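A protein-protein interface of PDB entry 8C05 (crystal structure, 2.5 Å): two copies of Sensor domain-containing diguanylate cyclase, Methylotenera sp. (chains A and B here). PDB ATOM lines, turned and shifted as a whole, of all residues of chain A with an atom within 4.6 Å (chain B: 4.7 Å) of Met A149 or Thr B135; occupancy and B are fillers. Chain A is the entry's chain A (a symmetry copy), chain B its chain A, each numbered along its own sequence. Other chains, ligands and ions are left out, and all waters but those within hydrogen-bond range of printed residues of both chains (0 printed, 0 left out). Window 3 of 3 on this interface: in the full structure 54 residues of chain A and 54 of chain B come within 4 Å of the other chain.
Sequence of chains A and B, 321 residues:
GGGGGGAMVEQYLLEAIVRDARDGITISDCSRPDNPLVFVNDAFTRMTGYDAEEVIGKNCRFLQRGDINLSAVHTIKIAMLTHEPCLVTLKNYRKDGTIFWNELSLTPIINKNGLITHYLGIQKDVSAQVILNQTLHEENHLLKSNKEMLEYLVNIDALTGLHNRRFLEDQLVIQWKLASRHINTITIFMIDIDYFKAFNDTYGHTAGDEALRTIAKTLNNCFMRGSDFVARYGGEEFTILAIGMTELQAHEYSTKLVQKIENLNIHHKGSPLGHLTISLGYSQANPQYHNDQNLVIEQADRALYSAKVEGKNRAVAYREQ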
ATOM      1  N   ASN A 146     -10.789  -8.075  -2.698  1.00  0.00           N
ATOM      2  CA  ASN A 146     -10.490  -8.570  -4.035  1.00  0.00           C
ATOM      3  C   ASN A 146     -11.569  -8.128  -5.013  1.00  0.00           C
ATOM      4  O   ASN A 146     -12.765  -8.230  -4.724  1.00  0.00           O
ATOM      5  CB  ASN A 146     -10.378 -10.095  -4.021  1.00  0.00           C
ATOM      6  CG  ASN A 146     -10.071 -10.670  -5.391  1.00  0.00           C
ATOM      7  OD1 ASN A 146      -9.461 -10.010  -6.233  1.00  0.00           O
ATOM      8  ND2 ASN A 146     -10.496 -11.907  -5.621  1.00  0.00           N
ATOM      9  N   LYS A 147     -11.143  -7.630  -6.177  1.00  0.00           N
ATOM     10  CA  LYS A 147     -12.097  -7.189  -7.190  1.00  0.00           C
ATOM     11  C   LYS A 147     -12.929  -8.357  -7.704  1.00  0.00           C
ATOM     12  O   LYS A 147     -14.157  -8.263  -7.808  1.00  0.00           O
ATOM     13  CB  LYS A 147     -11.362  -6.507  -8.345  1.00  0.00           C
ATOM     14  CG  LYS A 147     -10.620  -5.239  -7.962  1.00  0.00           C
ATOM     15  CD  LYS A 147      -9.962  -4.605  -9.179  1.00  0.00           C
ATOM     16  CE  LYS A 147      -9.250  -3.312  -8.816  1.00  0.00           C
ATOM     17  NZ  LYS A 147      -8.614  -2.676 -10.003  1.00  0.00           N
ATOM     18  N   GLU A 148     -12.272  -9.473  -8.029  1.00  0.00           N
ATOM     19  CA  GLU A 148     -12.985 -10.626  -8.567  1.00  0.00           C
ATOM     20  C   GLU A 148     -13.936 -11.230  -7.542  1.00  0.00           C
ATOM     21  O   GLU A 148     -14.970 -11.795  -7.917  1.00  0.00           O
ATOM     22  CB  GLU A 148     -11.985 -11.673  -9.055  1.00  0.00           C
ATOM     23  CG  GLU A 148     -10.910 -11.104  -9.965  1.00  0.00           C
ATOM     24  CD  GLU A 148      -9.871 -12.133 -10.355  1.00  0.00           C
ATOM     25  OE1 GLU A 148     -10.183 -13.342 -10.307  1.00  0.00           O
ATOM     26  OE2 GLU A 148      -8.740 -11.734 -10.705  1.00  0.00           O
ATOM     27  N   MET A 149     -13.610 -11.123  -6.252  1.00  0.00           N
ATOM     28  CA  MET A 149     -14.523 -11.600  -5.221  1.00  0.00           C
ATOM     29  C   MET A 149     -15.754 -10.708  -5.123  1.00  0.00           C
ATOM     30  O   MET A 149     -16.863 -11.195  -4.873  1.00  0.00           O
ATOM     31  CB  MET A 149     -13.806 -11.673  -3.873  1.00  0.00           C
ATOM     32  CG  MET A 149     -14.626 -12.324  -2.770  1.00  0.00           C
ATOM     33  SD  MET A 149     -13.881 -12.119  -1.142  1.00  0.00           S
ATOM     34  CE  MET A 149     -12.233 -12.752  -1.439  1.00  0.00           C
ATOM     35  N   LEU A 150     -15.579  -9.398  -5.318  1.00  0.00           N
ATOM     36  CA  LEU A 150     -16.719  -8.486  -5.278  1.00  0.00           C
ATOM     37  C   LEU A 150     -17.634  -8.696  -6.477  1.00  0.00           C
ATOM     38  O   LEU A 150     -18.858  -8.564  -6.360  1.00  0.00           O
ATOM     39  CB  LEU A 150     -16.231  -7.040  -5.215  1.00  0.00           C
ATOM     40  CG  LEU A 150     -15.481  -6.644  -3.941  1.00  0.00           C
ATOM     41  CD1 LEU A 150     -15.022  -5.197  -4.010  1.00  0.00           C
ATOM     42  CD2 LEU A 150     -16.350  -6.876  -2.712  1.00  0.00           C
ATOM     43  N   GLU A 151     -17.060  -9.020  -7.639  1.00  0.00           N
ATOM     44  CA  GLU A 151     -17.877  -9.357  -8.802  1.00  0.00           C
ATOM     45  C   GLU A 151     -18.710 -10.605  -8.548  1.00  0.00           C
ATOM     46  O   GLU A 151     -19.831 -10.720  -9.057  1.00  0.00           O
ATOM     47  CB  GLU A 151     -16.986  -9.553 -10.026  1.00  0.00           C
ATOM     48  CG  GLU A 151     -16.077  -8.374 -10.329  1.00  0.00           C
ATOM     49  CD  GLU A 151     -14.862  -8.770 -11.144  1.00  0.00           C
ATOM     50  OE1 GLU A 151     -14.746  -9.965 -11.491  1.00  0.00           O
ATOM     51  OE2 GLU A 151     -14.027  -7.891 -11.441  1.00  0.00           O
ATOM     52  N   TYR A 152     -18.179 -11.547  -7.768  1.00  0.00           N
ATOM     53  CA  TYR A 152     -18.938 -12.741  -7.412  1.00  0.00           C
ATOM     54  C   TYR A 152     -20.030 -12.416  -6.402  1.00  0.00           C
ATOM     55  O   TYR A 152     -21.151 -12.927  -6.504  1.00  0.00           O
ATOM     56  CB  TYR A 152     -17.991 -13.805  -6.863  1.00  0.00           C
ATOM     57  CG  TYR A 152     -18.649 -15.103  -6.463  1.00  0.00           C
ATOM     58  CD1 TYR A 152     -19.002 -16.050  -7.416  1.00  0.00           C
ATOM     59  CD2 TYR A 152     -18.899 -15.394  -5.128  1.00  0.00           C
ATOM     60  CE1 TYR A 152     -19.596 -17.243  -7.052  1.00  0.00           C
ATOM     61  CE2 TYR A 152     -19.493 -16.583  -4.755  1.00  0.00           C
ATOM     62  CZ  TYR A 152     -19.839 -17.504  -5.721  1.00  0.00           C
ATOM     63  OH  TYR A 152     -20.432 -18.691  -5.353  1.00  0.00           O
ATOM     64  N   LEU A 153     -19.724 -11.558  -5.427  1.00  0.00           N
ATOM     65  CA  LEU A 153     -20.682 -11.169  -4.399  1.00  0.00           C
ATOM     66  C   LEU A 153     -21.805 -10.288  -4.927  1.00  0.00           C
ATOM     67  O   LEU A 153     -22.694  -9.928  -4.147  1.00  0.00           O
ATOM     68  CB  LEU A 153     -19.957 -10.451  -3.258  1.00  0.00           C
ATOM     69  CG  LEU A 153     -19.251 -11.343  -2.237  1.00  0.00           C
ATOM     70  CD1 LEU A 153     -18.417 -10.511  -1.276  1.00  0.00           C
ATOM     71  CD2 LEU A 153     -20.275 -12.172  -1.477  1.00  0.00           C
ATOM     72  N   ILE B 131     -11.832 -17.901  -7.629  1.00  0.00           N
ATOM     73  CA  ILE B 131     -11.698 -16.991  -6.497  1.00  0.00           C
ATOM     74  C   ILE B 131     -11.169 -17.726  -5.272  1.00  0.00           C
ATOM     75  O   ILE B 131     -10.339 -17.195  -4.525  1.00  0.00           O
ATOM     76  CB  ILE B 131     -13.044 -16.302  -6.219  1.00  0.00           C
ATOM     77  CG1 ILE B 131     -13.445 -15.457  -7.427  1.00  0.00           C
ATOM     78  CG2 ILE B 131     -12.962 -15.446  -4.964  1.00  0.00           C
ATOM     79  CD1 ILE B 131     -14.922 -15.269  -7.571  1.00  0.00           C
ATOM     80  N   LEU B 132     -11.631 -18.958  -5.046  1.00  0.00           N
ATOM     81  CA  LEU B 132     -11.159 -19.716  -3.892  1.00  0.00           C
ATOM     82  C   LEU B 132      -9.686 -20.077  -4.037  1.00  0.00           C
ATOM     83  O   LEU B 132      -8.897 -19.895  -3.103  1.00  0.00           O
ATOM     84  CB  LEU B 132     -12.008 -20.974  -3.701  1.00  0.00           C
ATOM     85  CG  LEU B 132     -11.679 -21.820  -2.469  1.00  0.00           C
ATOM     86  CD1 LEU B 132     -11.849 -21.005  -1.196  1.00  0.00           C
ATOM     87  CD2 LEU B 132     -12.543 -23.072  -2.427  1.00  0.00           C
ATOM     88  N   ASN B 133      -9.294 -20.585  -5.210  1.00  0.00           N
ATOM     89  CA  ASN B 133      -7.904 -20.979  -5.420  1.00  0.00           C
ATOM     90  C   ASN B 133      -6.962 -19.781  -5.376  1.00  0.00           C
ATOM     91  O   ASN B 133      -5.800 -19.926  -4.980  1.00  0.00           O
ATOM     92  CB  ASN B 133      -7.762 -21.722  -6.749  1.00  0.00           C
ATOM     93  CG  ASN B 133      -8.513 -23.039  -6.761  1.00  0.00           C
ATOM     94  OD1 ASN B 133      -9.404 -23.266  -5.944  1.00  0.00           O
ATOM     95  ND2 ASN B 133      -8.156 -23.916  -7.692  1.00  0.00           N
ATOM     96  N   GLN B 134      -7.437 -18.600  -5.778  1.00  0.00           N
ATOM     97  CA  GLN B 134      -6.611 -17.402  -5.663  1.00  0.00           C
ATOM     98  C   GLN B 134      -6.407 -17.013  -4.205  1.00  0.00           C
ATOM     99  O   GLN B 134      -5.327 -16.543  -3.827  1.00  0.00           O
ATOM    100  CB  GLN B 134      -7.239 -16.249  -6.445  1.00  0.00           C
ATOM    101  CG  GLN B 134      -6.986 -16.301  -7.943  1.00  0.00           C
ATOM    102  CD  GLN B 134      -7.688 -15.183  -8.685  1.00  0.00           C
ATOM    103  OE1 GLN B 134      -8.669 -14.619  -8.200  1.00  0.00           O
ATOM    104  NE2 GLN B 134      -7.186 -14.851  -9.870  1.00  0.00           N
ATOM    105  N   THR B 135      -7.430 -17.201  -3.371  1.00  0.00           N
ATOM    106  CA  THR B 135      -7.317 -16.901  -1.950  1.00  0.00           C
ATOM    107  C   THR B 135      -6.568 -17.977  -1.174  1.00  0.00           C
ATOM    108  O   THR B 135      -6.327 -17.796   0.025  1.00  0.00           O
ATOM    109  CB  THR B 135      -8.706 -16.711  -1.335  1.00  0.00           C
ATOM    110  OG1 THR B 135      -9.513 -17.865  -1.607  1.00  0.00           O
ATOM    111  CG2 THR B 135      -9.383 -15.474  -1.911  1.00  0.00           C
ATOM    112  N   LEU B 136      -6.193 -19.082  -1.821  1.00  0.00           N
ATOM    113  CA  LEU B 136      -5.510 -20.156  -1.111  1.00  0.00           C
ATOM    114  C   LEU B 136      -4.054 -19.822  -0.819  1.00  0.00           C
ATOM    115  O   LEU B 136      -3.519 -20.266   0.203  1.00  0.00           O
ATOM    116  CB  LEU B 136      -5.602 -21.459  -1.905  1.00  0.00           C
ATOM    117  CG  LEU B 136      -6.979 -22.123  -1.934  1.00  0.00           C
ATOM    118  CD1 LEU B 136      -6.941 -23.409  -2.740  1.00  0.00           C
ATOM    119  CD2 LEU B 136      -7.480 -22.384  -0.521  1.00  0.00           C
ATOM    120  N   HIS B 137      -3.392 -19.055  -1.690  1.00  0.00           N
ATOM    121  CA  HIS B 137      -2.005 -18.698  -1.421  1.00  0.00           C
ATOM    122  C   HIS B 137      -1.893 -17.670  -0.303  1.00  0.00           C
ATOM    123  O   HIS B 137      -0.845 -17.591   0.347  1.00  0.00           O
ATOM    124  CB  HIS B 137      -1.320 -18.199  -2.697  1.00  0.00           C
ATOM    125  CG  HIS B 137      -1.667 -16.791  -3.076  1.00  0.00           C
ATOM    126  ND1 HIS B 137      -2.631 -16.489  -4.012  1.00  0.00           N
ATOM    127  CD2 HIS B 137      -1.155 -15.606  -2.669  1.00  0.00           C
ATOM    128  CE1 HIS B 137      -2.708 -15.178  -4.155  1.00  0.00           C
ATOM    129  NE2 HIS B 137      -1.824 -14.619  -3.350  1.00  0.00           N
ATOM    130  N   GLU B 138      -2.943 -16.891  -0.065  1.00  0.00           N
ATOM    131  CA  GLU B 138      -3.042 -16.139   1.172  1.00  0.00           C
ATOM    132  C   GLU B 138      -3.544 -17.052   2.287  1.00  0.00           C
ATOM    133  O   GLU B 138      -4.089 -18.133   2.042  1.00  0.00           O
ATOM    134  CB  GLU B 138      -3.979 -14.940   1.019  1.00  0.00           C
ATOM    135  CG  GLU B 138      -3.462 -13.834   0.114  1.00  0.00           C
ATOM    136  CD  GLU B 138      -4.031 -13.908  -1.289  1.00  0.00           C
ATOM    137  OE1 GLU B 138      -4.855 -14.807  -1.551  1.00  0.00           O
ATOM    138  OE2 GLU B 138      -3.655 -13.065  -2.129  1.00  0.00           O
ATOM    139  N   ASN B 140      -6.021 -16.376   4.490  1.00  0.00           N
ATOM    140  CA  ASN B 140      -7.481 -16.327   4.431  1.00  0.00           C
ATOM    141  C   ASN B 140      -8.129 -16.959   5.661  1.00  0.00           C
ATOM    142  O   ASN B 140      -8.700 -18.047   5.584  1.00  0.00           O
ATOM    143  CB  ASN B 140      -7.990 -17.014   3.160  1.00  0.00           C
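The side-chain carboxylate (OE1) of Glu A148 sits close to the side-chain amide oxygen (OE1) of Gln B134, at 2.9 Å.
O of Ile B131 sits at hydrogen-bond distance from OG1 of Thr B135 (3.1 Å).
O of Leu B132 is in hydrogen-bond range of OG1 of Thr B135 (2.6 Å).
The backbone carbonyl oxygen (O) of Gln B134 lies within hydrogen-bond range of a ring nitrogen (ND1) of His B137 (2.7 Å).
The side-chain amide oxygen (OD1) of Asn A146 lies close to the backbone NH (N) of Glu A148 (3.4 Å).
N of Met A149 sits close to ND2 of Asn A146 (3.3 Å).
Ile B131 touches Glu A148 (CD1 to O, 3.5 Å).
Thr B135 touches Met A149.
CD1 of Ile B131 touches CB of Tyr A152, at 3.5 Å.
Printed residues of chain B within 4 Å of Glu A148: Ile B131 and Gln B134.
Printed residues of chain B within 4 Å of Met A149: Thr B135.
Printed residues of chain A within 4 Å of Gln B134: Glu A148.
The nearest printed residue of chain A that does not touch Thr B135 is Asn A146 (5.3 Å).
The nearest printed residue of chain A that does not touch Ile B131 is Met A149 (4.02 Å).
Printed residues of chain B that touch a printed residue of chain A: Ile B131, Gln B134 and Thr B135.
Hydrophobic or aromatic side chains of chain B within 4 Å of the printed part of chain A: Ile B131.
Printed residues of chain A that touch a printed residue of chain B: Glu A148, Met A149 and Tyr A152.
Hydrophobic or aromatic side chains of chain A that line the printed part of chain B: Met A149 and Tyr A152.
Along chain A the printed residues that touch a printed residue of chain B span positions 148 to 152.
Among the printed residues, 4 pairs touch across the chains.
Among the printed residues, no Asp or Glu carboxylate lies within 4 Å of a Lys or Arg side-chain nitrogen of the other chain.
No position is printed for both chains.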
